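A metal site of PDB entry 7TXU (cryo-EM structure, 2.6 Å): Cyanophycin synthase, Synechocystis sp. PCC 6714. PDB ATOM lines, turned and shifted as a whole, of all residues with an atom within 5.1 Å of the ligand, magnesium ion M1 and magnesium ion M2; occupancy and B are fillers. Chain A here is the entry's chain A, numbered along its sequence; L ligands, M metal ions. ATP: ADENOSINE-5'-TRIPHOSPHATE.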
ATOM      1  N   GLY A 495      23.691  -8.174 -22.430  1.00  0.00           N
ATOM      2  CA  GLY A 495      23.854  -6.737 -22.203  1.00  0.00           C
ATOM      3  C   GLY A 495      24.459  -6.472 -20.841  1.00  0.00           C
ATOM      4  O   GLY A 495      24.471  -7.356 -20.003  1.00  0.00           O
ATOM      5  N   THR A 496      24.987  -5.283 -20.611  1.00  0.00           N
ATOM      6  CA  THR A 496      25.626  -4.994 -19.318  1.00  0.00           C
ATOM      7  C   THR A 496      24.701  -4.999 -18.112  1.00  0.00           C
ATOM      8  O   THR A 496      25.056  -5.615 -17.104  1.00  0.00           O
ATOM      9  CB  THR A 496      26.416  -3.660 -19.330  1.00  0.00           C
ATOM     10  OG1 THR A 496      27.470  -3.716 -20.304  1.00  0.00           O
ATOM     11  CG2 THR A 496      27.063  -3.441 -17.960  1.00  0.00           C
ATOM     12  N   ASN A 497      23.516  -4.375 -18.200  1.00  0.00           N
ATOM     13  CA  ASN A 497      22.549  -4.342 -17.088  1.00  0.00           C
ATOM     14  C   ASN A 497      21.131  -4.720 -17.541  1.00  0.00           C
ATOM     15  O   ASN A 497      20.707  -4.347 -18.625  1.00  0.00           O
ATOM     16  CB  ASN A 497      22.490  -2.969 -16.443  1.00  0.00           C
ATOM     17  CG  ASN A 497      23.767  -2.476 -15.780  1.00  0.00           C
ATOM     18  OD1 ASN A 497      24.293  -3.069 -14.850  1.00  0.00           O
ATOM     19  ND2 ASN A 497      24.263  -1.361 -16.216  1.00  0.00           N
ATOM     20  N   GLY A 498      20.365  -5.389 -16.681  1.00  0.00           N
ATOM     21  CA  GLY A 498      18.951  -5.716 -16.944  1.00  0.00           C
ATOM     22  C   GLY A 498      18.598  -7.131 -17.432  1.00  0.00           C
ATOM     23  O   GLY A 498      17.419  -7.485 -17.541  1.00  0.00           O
ATOM     24  N   LYS A 499      19.608  -7.970 -17.666  1.00  0.00           N
ATOM     25  CA  LYS A 499      19.425  -9.341 -18.151  1.00  0.00           C
ATOM     26  C   LYS A 499      18.523 -10.241 -17.334  1.00  0.00           C
ATOM     27  O   LYS A 499      17.673 -10.920 -17.908  1.00  0.00           O
ATOM     28  CB  LYS A 499      20.761 -10.043 -18.235  1.00  0.00           C
ATOM     29  CG  LYS A 499      21.721  -9.540 -19.247  1.00  0.00           C
ATOM     30  CD  LYS A 499      23.026 -10.410 -19.285  1.00  0.00           C
ATOM     31  CE  LYS A 499      23.896 -10.228 -18.093  1.00  0.00           C
ATOM     32  NZ  LYS A 499      24.389  -8.876 -18.051  1.00  0.00           N
ATOM     33  N   THR A 500      18.696 -10.281 -16.025  1.00  0.00           N
ATOM     34  CA  THR A 500      17.912 -11.176 -15.177  1.00  0.00           C
ATOM     35  C   THR A 500      16.443 -10.813 -15.156  1.00  0.00           C
ATOM     36  O   THR A 500      15.582 -11.697 -15.187  1.00  0.00           O
ATOM     37  CB  THR A 500      18.486 -11.232 -13.751  1.00  0.00           C
ATOM     38  OG1 THR A 500      19.847 -11.761 -13.815  1.00  0.00           O
ATOM     39  CG2 THR A 500      17.653 -12.105 -12.839  1.00  0.00           C
ATOM     40  N   THR A 501      16.140  -9.531 -15.094  1.00  0.00           N
ATOM     41  CA  THR A 501      14.771  -9.048 -15.085  1.00  0.00           C
ATOM     42  C   THR A 501      14.070  -9.359 -16.407  1.00  0.00           C
ATOM     43  O   THR A 501      12.932  -9.810 -16.411  1.00  0.00           O
ATOM     44  CB  THR A 501      14.718  -7.541 -14.838  1.00  0.00           C
ATOM     45  OG1 THR A 501      15.310  -7.239 -13.568  1.00  0.00           O
ATOM     46  CG2 THR A 501      13.299  -7.077 -14.823  1.00  0.00           C
ATOM     47  N   THR A 522      21.196 -15.916 -13.090  1.00  0.00           N
ATOM     48  CA  THR A 522      22.200 -15.810 -12.038  1.00  0.00           C
ATOM     49  C   THR A 522      21.702 -16.248 -10.648  1.00  0.00           C
ATOM     50  O   THR A 522      22.483 -16.264  -9.698  1.00  0.00           O
ATOM     51  CB  THR A 522      22.825 -14.406 -11.967  1.00  0.00           C
ATOM     52  OG1 THR A 522      21.804 -13.395 -11.948  1.00  0.00           O
ATOM     53  CG2 THR A 522      23.733 -14.195 -13.084  1.00  0.00           C
ATOM     54  N   GLU A 558      19.893 -16.335 -19.903  1.00  0.00           N
ATOM     55  CA  GLU A 558      20.631 -15.058 -19.818  1.00  0.00           C
ATOM     56  C   GLU A 558      22.094 -15.403 -20.093  1.00  0.00           C
ATOM     57  O   GLU A 558      22.615 -16.370 -19.539  1.00  0.00           O
ATOM     58  CB  GLU A 558      20.465 -14.268 -18.472  1.00  0.00           C
ATOM     59  CG  GLU A 558      21.401 -14.537 -17.328  1.00  0.00           C
ATOM     60  CD  GLU A 558      21.206 -13.661 -15.975  1.00  0.00           C
ATOM     61  OE1 GLU A 558      20.296 -13.910 -15.229  1.00  0.00           O
ATOM     62  OE2 GLU A 558      22.027 -12.806 -15.654  1.00  0.00           O
ATOM     63  N   ASN A 581      22.144  -3.322 -23.789  1.00  0.00           N
ATOM     64  CA  ASN A 581      22.980  -2.141 -23.595  1.00  0.00           C
ATOM     65  C   ASN A 581      24.449  -2.485 -23.465  1.00  0.00           C
ATOM     66  O   ASN A 581      24.796  -3.585 -23.014  1.00  0.00           O
ATOM     67  CB  ASN A 581      22.513  -1.331 -22.380  1.00  0.00           C
ATOM     68  CG  ASN A 581      22.392  -2.117 -21.103  1.00  0.00           C
ATOM     69  OD1 ASN A 581      23.365  -2.569 -20.510  1.00  0.00           O
ATOM     70  ND2 ASN A 581      21.191  -2.316 -20.679  1.00  0.00           N
ATOM     71  N   ASP A 585      31.307  -1.665 -17.359  1.00  0.00           N
ATOM     72  CA  ASP A 585      31.475  -2.462 -16.140  1.00  0.00           C
ATOM     73  C   ASP A 585      32.421  -3.574 -16.502  1.00  0.00           C
ATOM     74  O   ASP A 585      32.602  -3.859 -17.685  1.00  0.00           O
ATOM     75  CB  ASP A 585      30.185  -3.045 -15.552  1.00  0.00           C
ATOM     76  CG  ASP A 585      30.384  -3.538 -14.007  1.00  0.00           C
ATOM     77  OD1 ASP A 585      31.517  -3.449 -13.509  1.00  0.00           O
ATOM     78  OD2 ASP A 585      29.400  -3.936 -13.357  1.00  0.00           O
ATOM     79  N   HIS A 586      33.056  -4.159 -15.520  1.00  0.00           N
ATOM     80  CA  HIS A 586      33.972  -5.266 -15.703  1.00  0.00           C
ATOM     81  C   HIS A 586      35.138  -4.947 -16.625  1.00  0.00           C
ATOM     82  O   HIS A 586      35.656  -5.845 -17.300  1.00  0.00           O
ATOM     83  CB  HIS A 586      33.259  -6.478 -16.318  1.00  0.00           C
ATOM     84  CG  HIS A 586      32.077  -7.009 -15.588  1.00  0.00           C
ATOM     85  ND1 HIS A 586      32.183  -7.688 -14.407  1.00  0.00           N
ATOM     86  CD2 HIS A 586      30.770  -6.986 -15.900  1.00  0.00           C
ATOM     87  CE1 HIS A 586      30.993  -8.065 -13.996  1.00  0.00           C
ATOM     88  NE2 HIS A 586      30.076  -7.662 -14.902  1.00  0.00           N
ATOM     89  N   PHE A 692      13.902   2.501 -16.421  1.00  0.00           N
ATOM     90  CA  PHE A 692      14.724   1.352 -16.728  1.00  0.00           C
ATOM     91  C   PHE A 692      13.905   0.070 -16.713  1.00  0.00           C
ATOM     92  O   PHE A 692      14.248  -0.888 -17.406  1.00  0.00           O
ATOM     93  CB  PHE A 692      15.915   1.356 -15.772  1.00  0.00           C
ATOM     94  CG  PHE A 692      15.566   1.246 -14.336  1.00  0.00           C
ATOM     95  CD1 PHE A 692      15.253   2.380 -13.602  1.00  0.00           C
ATOM     96  CD2 PHE A 692      15.605   0.051 -13.687  1.00  0.00           C
ATOM     97  CE1 PHE A 692      14.964   2.306 -12.284  1.00  0.00           C
ATOM     98  CE2 PHE A 692      15.321  -0.019 -12.348  1.00  0.00           C
ATOM     99  CZ  PHE A 692      15.006   1.113 -11.660  1.00  0.00           C
ATOM    100  N   MET A 693      12.782   0.057 -15.995  1.00  0.00           N
ATOM    101  CA  MET A 693      11.946  -1.113 -15.953  1.00  0.00           C
ATOM    102  C   MET A 693      11.070  -1.112 -17.181  1.00  0.00           C
ATOM    103  O   MET A 693      10.770  -2.170 -17.740  1.00  0.00           O
ATOM    104  CB  MET A 693      11.135  -1.123 -14.676  1.00  0.00           C
ATOM    105  CG  MET A 693      11.982  -1.259 -13.431  1.00  0.00           C
ATOM    106  SD  MET A 693      12.962  -2.781 -13.338  1.00  0.00           S
ATOM    107  CE  MET A 693      11.700  -3.934 -12.908  1.00  0.00           C
ATOM    108  N   ASN A 696      13.046  -2.552 -20.096  1.00  0.00           N
ATOM    109  CA  ASN A 696      13.146  -4.008 -20.079  1.00  0.00           C
ATOM    110  C   ASN A 696      11.842  -4.665 -20.501  1.00  0.00           C
ATOM    111  O   ASN A 696      11.859  -5.680 -21.204  1.00  0.00           O
ATOM    112  CB  ASN A 696      13.517  -4.463 -18.711  1.00  0.00           C
ATOM    113  CG  ASN A 696      14.859  -4.132 -18.447  1.00  0.00           C
ATOM    114  OD1 ASN A 696      15.726  -4.097 -19.317  1.00  0.00           O
ATOM    115  ND2 ASN A 696      15.097  -3.809 -17.268  1.00  0.00           N
ATOM    116  N   GLY A 730      16.883  -7.704  -3.595  1.00  0.00           N
ATOM    117  CA  GLY A 730      17.894  -6.768  -4.053  1.00  0.00           C
ATOM    118  C   GLY A 730      17.573  -6.091  -5.368  1.00  0.00           C
ATOM    119  O   GLY A 730      18.387  -5.343  -5.899  1.00  0.00           O
ATOM    120  N   ARG A 731      16.400  -6.376  -5.943  1.00  0.00           N
ATOM    121  CA  ARG A 731      16.047  -5.774  -7.219  1.00  0.00           C
ATOM    122  C   ARG A 731      14.736  -5.017  -7.095  1.00  0.00           C
ATOM    123  O   ARG A 731      13.671  -5.613  -7.263  1.00  0.00           O
ATOM    124  CB  ARG A 731      15.928  -6.855  -8.279  1.00  0.00           C
ATOM    125  CG  ARG A 731      17.192  -7.683  -8.505  1.00  0.00           C
ATOM    126  CD  ARG A 731      17.025  -8.675  -9.597  1.00  0.00           C
ATOM    127  NE  ARG A 731      18.246  -9.482  -9.817  1.00  0.00           N
ATOM    128  CZ  ARG A 731      18.521 -10.683  -9.177  1.00  0.00           C
ATOM    129  NH1 ARG A 731      17.716 -11.205  -8.301  1.00  0.00           N
ATOM    130  NH2 ARG A 731      19.595 -11.385  -9.437  1.00  0.00           N
ATOM    131  N   MET A 732      14.801  -3.718  -6.788  1.00  0.00           N
ATOM    132  CA  MET A 732      13.638  -2.874  -6.514  1.00  0.00           C
ATOM    133  C   MET A 732      12.655  -3.416  -5.470  1.00  0.00           C
ATOM    134  O   MET A 732      11.493  -3.645  -5.787  1.00  0.00           O
ATOM    135  CB  MET A 732      12.893  -2.562  -7.814  1.00  0.00           C
ATOM    136  CG  MET A 732      13.714  -1.761  -8.812  1.00  0.00           C
ATOM    137  SD  MET A 732      14.194  -0.119  -8.199  1.00  0.00           S
ATOM    138  CE  MET A 732      12.691   0.827  -8.258  1.00  0.00           C
ATOM    139  N   ASP A 745      17.872  -2.142  -3.012  1.00  0.00           N
ATOM    140  CA  ASP A 745      18.330  -2.516  -4.348  1.00  0.00           C
ATOM    141  C   ASP A 745      19.812  -2.871  -4.281  1.00  0.00           C
ATOM    142  O   ASP A 745      20.381  -2.911  -3.187  1.00  0.00           O
ATOM    143  CB  ASP A 745      18.062  -1.394  -5.358  1.00  0.00           C
ATOM    144  CG  ASP A 745      17.865  -1.903  -6.808  1.00  0.00           C
ATOM    145  OD1 ASP A 745      18.780  -2.413  -7.445  1.00  0.00           O
ATOM    146  OD2 ASP A 745      16.775  -1.822  -7.247  1.00  0.00           O
ATOM    147  N   TYR A 746      20.408  -3.217  -5.412  1.00  0.00           N
ATOM    148  CA  TYR A 746      21.808  -3.592  -5.386  1.00  0.00           C
ATOM    149  C   TYR A 746      22.509  -3.178  -6.662  1.00  0.00           C
ATOM    150  O   TYR A 746      22.700  -3.982  -7.583  1.00  0.00           O
ATOM    151  CB  TYR A 746      21.963  -5.094  -5.187  1.00  0.00           C
ATOM    152  CG  TYR A 746      23.325  -5.456  -4.666  1.00  0.00           C
ATOM    153  CD1 TYR A 746      23.565  -5.230  -3.340  1.00  0.00           C
ATOM    154  CD2 TYR A 746      24.320  -5.994  -5.476  1.00  0.00           C
ATOM    155  CE1 TYR A 746      24.754  -5.539  -2.795  1.00  0.00           C
ATOM    156  CE2 TYR A 746      25.551  -6.298  -4.919  1.00  0.00           C
ATOM    157  CZ  TYR A 746      25.759  -6.082  -3.556  1.00  0.00           C
ATOM    158  OH  TYR A 746      26.970  -6.369  -2.941  1.00  0.00           O
ATOM    159  N   ALA A 747      22.857  -1.917  -6.733  1.00  0.00           N
ATOM    160  CA  ALA A 747      23.537  -1.359  -7.885  1.00  0.00           C
ATOM    161  C   ALA A 747      24.984  -1.831  -7.811  1.00  0.00           C
ATOM    162  O   ALA A 747      25.498  -2.046  -6.716  1.00  0.00           O
ATOM    163  CB  ALA A 747      23.429   0.148  -7.886  1.00  0.00           C
ATOM    164  N   ALA A 751      25.808   2.836 -13.534  1.00  0.00           N
ATOM    165  CA  ALA A 751      24.542   2.986 -14.238  1.00  0.00           C
ATOM    166  C   ALA A 751      23.391   2.611 -13.328  1.00  0.00           C
ATOM    167  O   ALA A 751      22.276   3.085 -13.532  1.00  0.00           O
ATOM    168  CB  ALA A 751      24.500   2.134 -15.477  1.00  0.00           C
ATOM    169  N   GLY A 752      23.617   1.734 -12.346  1.00  0.00           N
ATOM    170  CA  GLY A 752      22.541   1.336 -11.474  1.00  0.00           C
ATOM    171  C   GLY A 752      22.288   2.329 -10.366  1.00  0.00           C
ATOM    172  O   GLY A 752      21.242   2.295  -9.709  1.00  0.00           O
ATOM    173  N   ALA A 755      20.101   4.669 -12.437  1.00  0.00           N
ATOM    174  CA  ALA A 755      18.772   4.126 -12.673  1.00  0.00           C
ATOM    175  C   ALA A 755      17.898   4.223 -11.427  1.00  0.00           C
ATOM    176  O   ALA A 755      16.750   4.683 -11.499  1.00  0.00           O
ATOM    177  CB  ALA A 755      18.912   2.675 -13.104  1.00  0.00           C
ATOM    178  N   VAL A 756      18.471   3.921 -10.265  1.00  0.00           N
ATOM    179  CA  VAL A 756      17.693   4.034  -9.055  1.00  0.00           C
ATOM    180  C   VAL A 756      17.437   5.497  -8.756  1.00  0.00           C
ATOM    181  O   VAL A 756      16.324   5.834  -8.339  1.00  0.00           O
ATOM    182  CB  VAL A 756      18.346   3.308  -7.875  1.00  0.00           C
ATOM    183  CG1 VAL A 756      17.588   3.589  -6.596  1.00  0.00           C
ATOM    184  CG2 VAL A 756      18.323   1.798  -8.150  1.00  0.00           C
HETATM  185  PG  ATP L   1      24.217  -9.586 -13.174  1.00  0.00           P
HETATM  186  O1G ATP L   1      23.356 -10.816 -13.471  1.00  0.00           O
HETATM  187  O2G ATP L   1      24.775  -9.686 -11.713  1.00  0.00           O
HETATM  188  O3G ATP L   1      25.481  -9.596 -14.109  1.00  0.00           O
HETATM  189  PB  ATP L   1      22.103  -8.271 -14.206  1.00  0.00           P
HETATM  190  O1B ATP L   1      22.622  -8.242 -15.558  1.00  0.00           O
HETATM  191  O2B ATP L   1      21.316  -9.677 -14.061  1.00  0.00           O
HETATM  192  O3B ATP L   1      23.376  -8.218 -13.214  1.00  0.00           O
HETATM  193  PA  ATP L   1      19.977  -7.115 -12.899  1.00  0.00           P
HETATM  194  O1A ATP L   1      19.973  -8.429 -12.234  1.00  0.00           O
HETATM  195  O2A ATP L   1      18.573  -6.978 -13.563  1.00  0.00           O
HETATM  196  O3A ATP L   1      21.130  -7.008 -14.037  1.00  0.00           O
HETATM  197  O5' ATP L   1      20.113  -5.952 -11.792  1.00  0.00           O
HETATM  198  C5' ATP L   1      20.798  -4.713 -12.211  1.00  0.00           C
HETATM  199  C4' ATP L   1      20.475  -3.589 -11.207  1.00  0.00           C
HETATM  200  O4' ATP L   1      21.111  -2.377 -11.707  1.00  0.00           O
HETATM  201  C3' ATP L   1      18.946  -3.291 -11.062  1.00  0.00           C
HETATM  202  O3' ATP L   1      18.404  -3.735  -9.800  1.00  0.00           O
HETATM  203  C2' ATP L   1      18.842  -1.766 -11.189  1.00  0.00           C
HETATM  204  O2' ATP L   1      18.830  -1.184  -9.870  1.00  0.00           O
HETATM  205  C1' ATP L   1      20.125  -1.353 -11.992  1.00  0.00           C
HETATM  206  N9  ATP L   1      19.988  -1.136 -13.490  1.00  0.00           N
HETATM  207  C8  ATP L   1      20.732  -0.265 -14.282  1.00  0.00           C
HETATM  208  N7  ATP L   1      20.341  -0.247 -15.531  1.00  0.00           N
HETATM  209  C5  ATP L   1      19.332  -1.113 -15.655  1.00  0.00           C
HETATM  210  C6  ATP L   1      18.498  -1.549 -16.746  1.00  0.00           C
HETATM  211  N6  ATP L   1      18.676  -1.038 -17.989  1.00  0.00           N
HETATM  212  N1  ATP L   1      17.513  -2.486 -16.505  1.00  0.00           N
HETATM  213  C2  ATP L   1      17.327  -3.010 -15.245  1.00  0.00           C
HETATM  214  N3  ATP L   1      18.081  -2.634 -14.208  1.00  0.00           N
HETATM  215  C4  ATP L   1      19.085  -1.707 -14.349  1.00  0.00           C
HETATM  216 MG    MG M   1      21.912 -11.961 -14.021  1.00  0.00          MG
HETATM  217 MG    MG M   2      27.684  -8.535 -14.649  1.00  0.00          MG
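The backbone NH of Met 732 lies within hydrogen-bond range of the side-chain carboxylate of Asp 745 (2.8 Å). The side-chain amide nitrogen of Asn 581 sits at hydrogen-bond distance from the backbone carbonyl oxygen of Asn 497. The backbone carbonyl oxygen (O) of Thr 496 sits at hydrogen-bond distance from the side-chain amino group (NZ) of Lys 499 (3.5 Å). N of Thr 496 sits at hydrogen-bond distance from O of Asn 581 (2.9 Å). The side-chain amino group (NZ) of Lys 499 is in hydrogen-bond range of the backbone carbonyl oxygen (O) of Gly 495. O of Phe 692 is in hydrogen-bond range of ND2 of Asn 696.
Of the 25 residues printed, 1 comes within 4 Å of magnesium ion M2. The nearest printed residue that does not touch magnesium ion M2 is Thr 496 (4.6 Å).
An oxygen (O2') of the ligand lies within hydrogen-bond range of the side-chain carboxylate (OD1) of Asp 745, at 2.7 Å. O2A of the ligand sits at hydrogen-bond distance from OG1 of Thr 501 (3.3 Å). The side-chain amino group (NZ) of Lys 499 lies within salt-bridge range of an oxygen (O1B) of the ligand (3.1 Å). The guanidinium group of Arg 731 is in salt-bridge range of an oxygen (O1A) of the ligand (3.2 Å). N of Gly 498 lies within hydrogen-bond range of O3A of the ligand (3.2 Å). N1 of the ligand sits at hydrogen-bond distance from ND2 of Asn 696. The backbone NH of Thr 500 sits close to an oxygen (O2B) of the ligand (3.3 Å).
Magnesium ion M1 is bound by OE2 of Glu 558 (1.8 Å), O1G of the ligand (1.9 Å), OG1 of Thr 500 (2.1 Å), O2B of the ligand (2.4 Å) and OG1 of Thr 522 (2.5 Å). Magnesium ion M1 has five donor atoms within binding distance. Slightly farther from magnesium ion M1 lies OE1 of Glu 558 (2.8 Å).
Magnesium ion M2 is bound by an oxygen (O3G) of the ligand (2.5 Å) and a ring nitrogen (NE2) of His 586 (2.6 Å). Magnesium ion M2 has two donor atoms within binding distance.
Merely in contact with the ligand: Thr 496 (3.9 Å), Asn 497 (3.6 Å), Asn 581 (3.9 Å), Phe 692 (3.7 Å), Ala 751 (3.8 Å), Gly 752 (3.7 Å), Ala 755 (3.7 Å) and Val 756 (3.5 Å). Hydrophobic or aromatic side chains within 4 Å of the ligand: Phe 692, Ala 755 and Val 756. 17 residues have an atom within 4 Å of the ligand: Thr 496, Asn 497, Gly 498, Lys 499, Thr 500, Thr 501, Thr 522, Glu 558, Asn 581, Phe 692, Asn 696, Arg 731, Asp 745, Ala 751, Gly 752, Ala 755 and Val 756. The nearest printed residue that does not touch the ligand is Gly 730 (4.2 Å).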
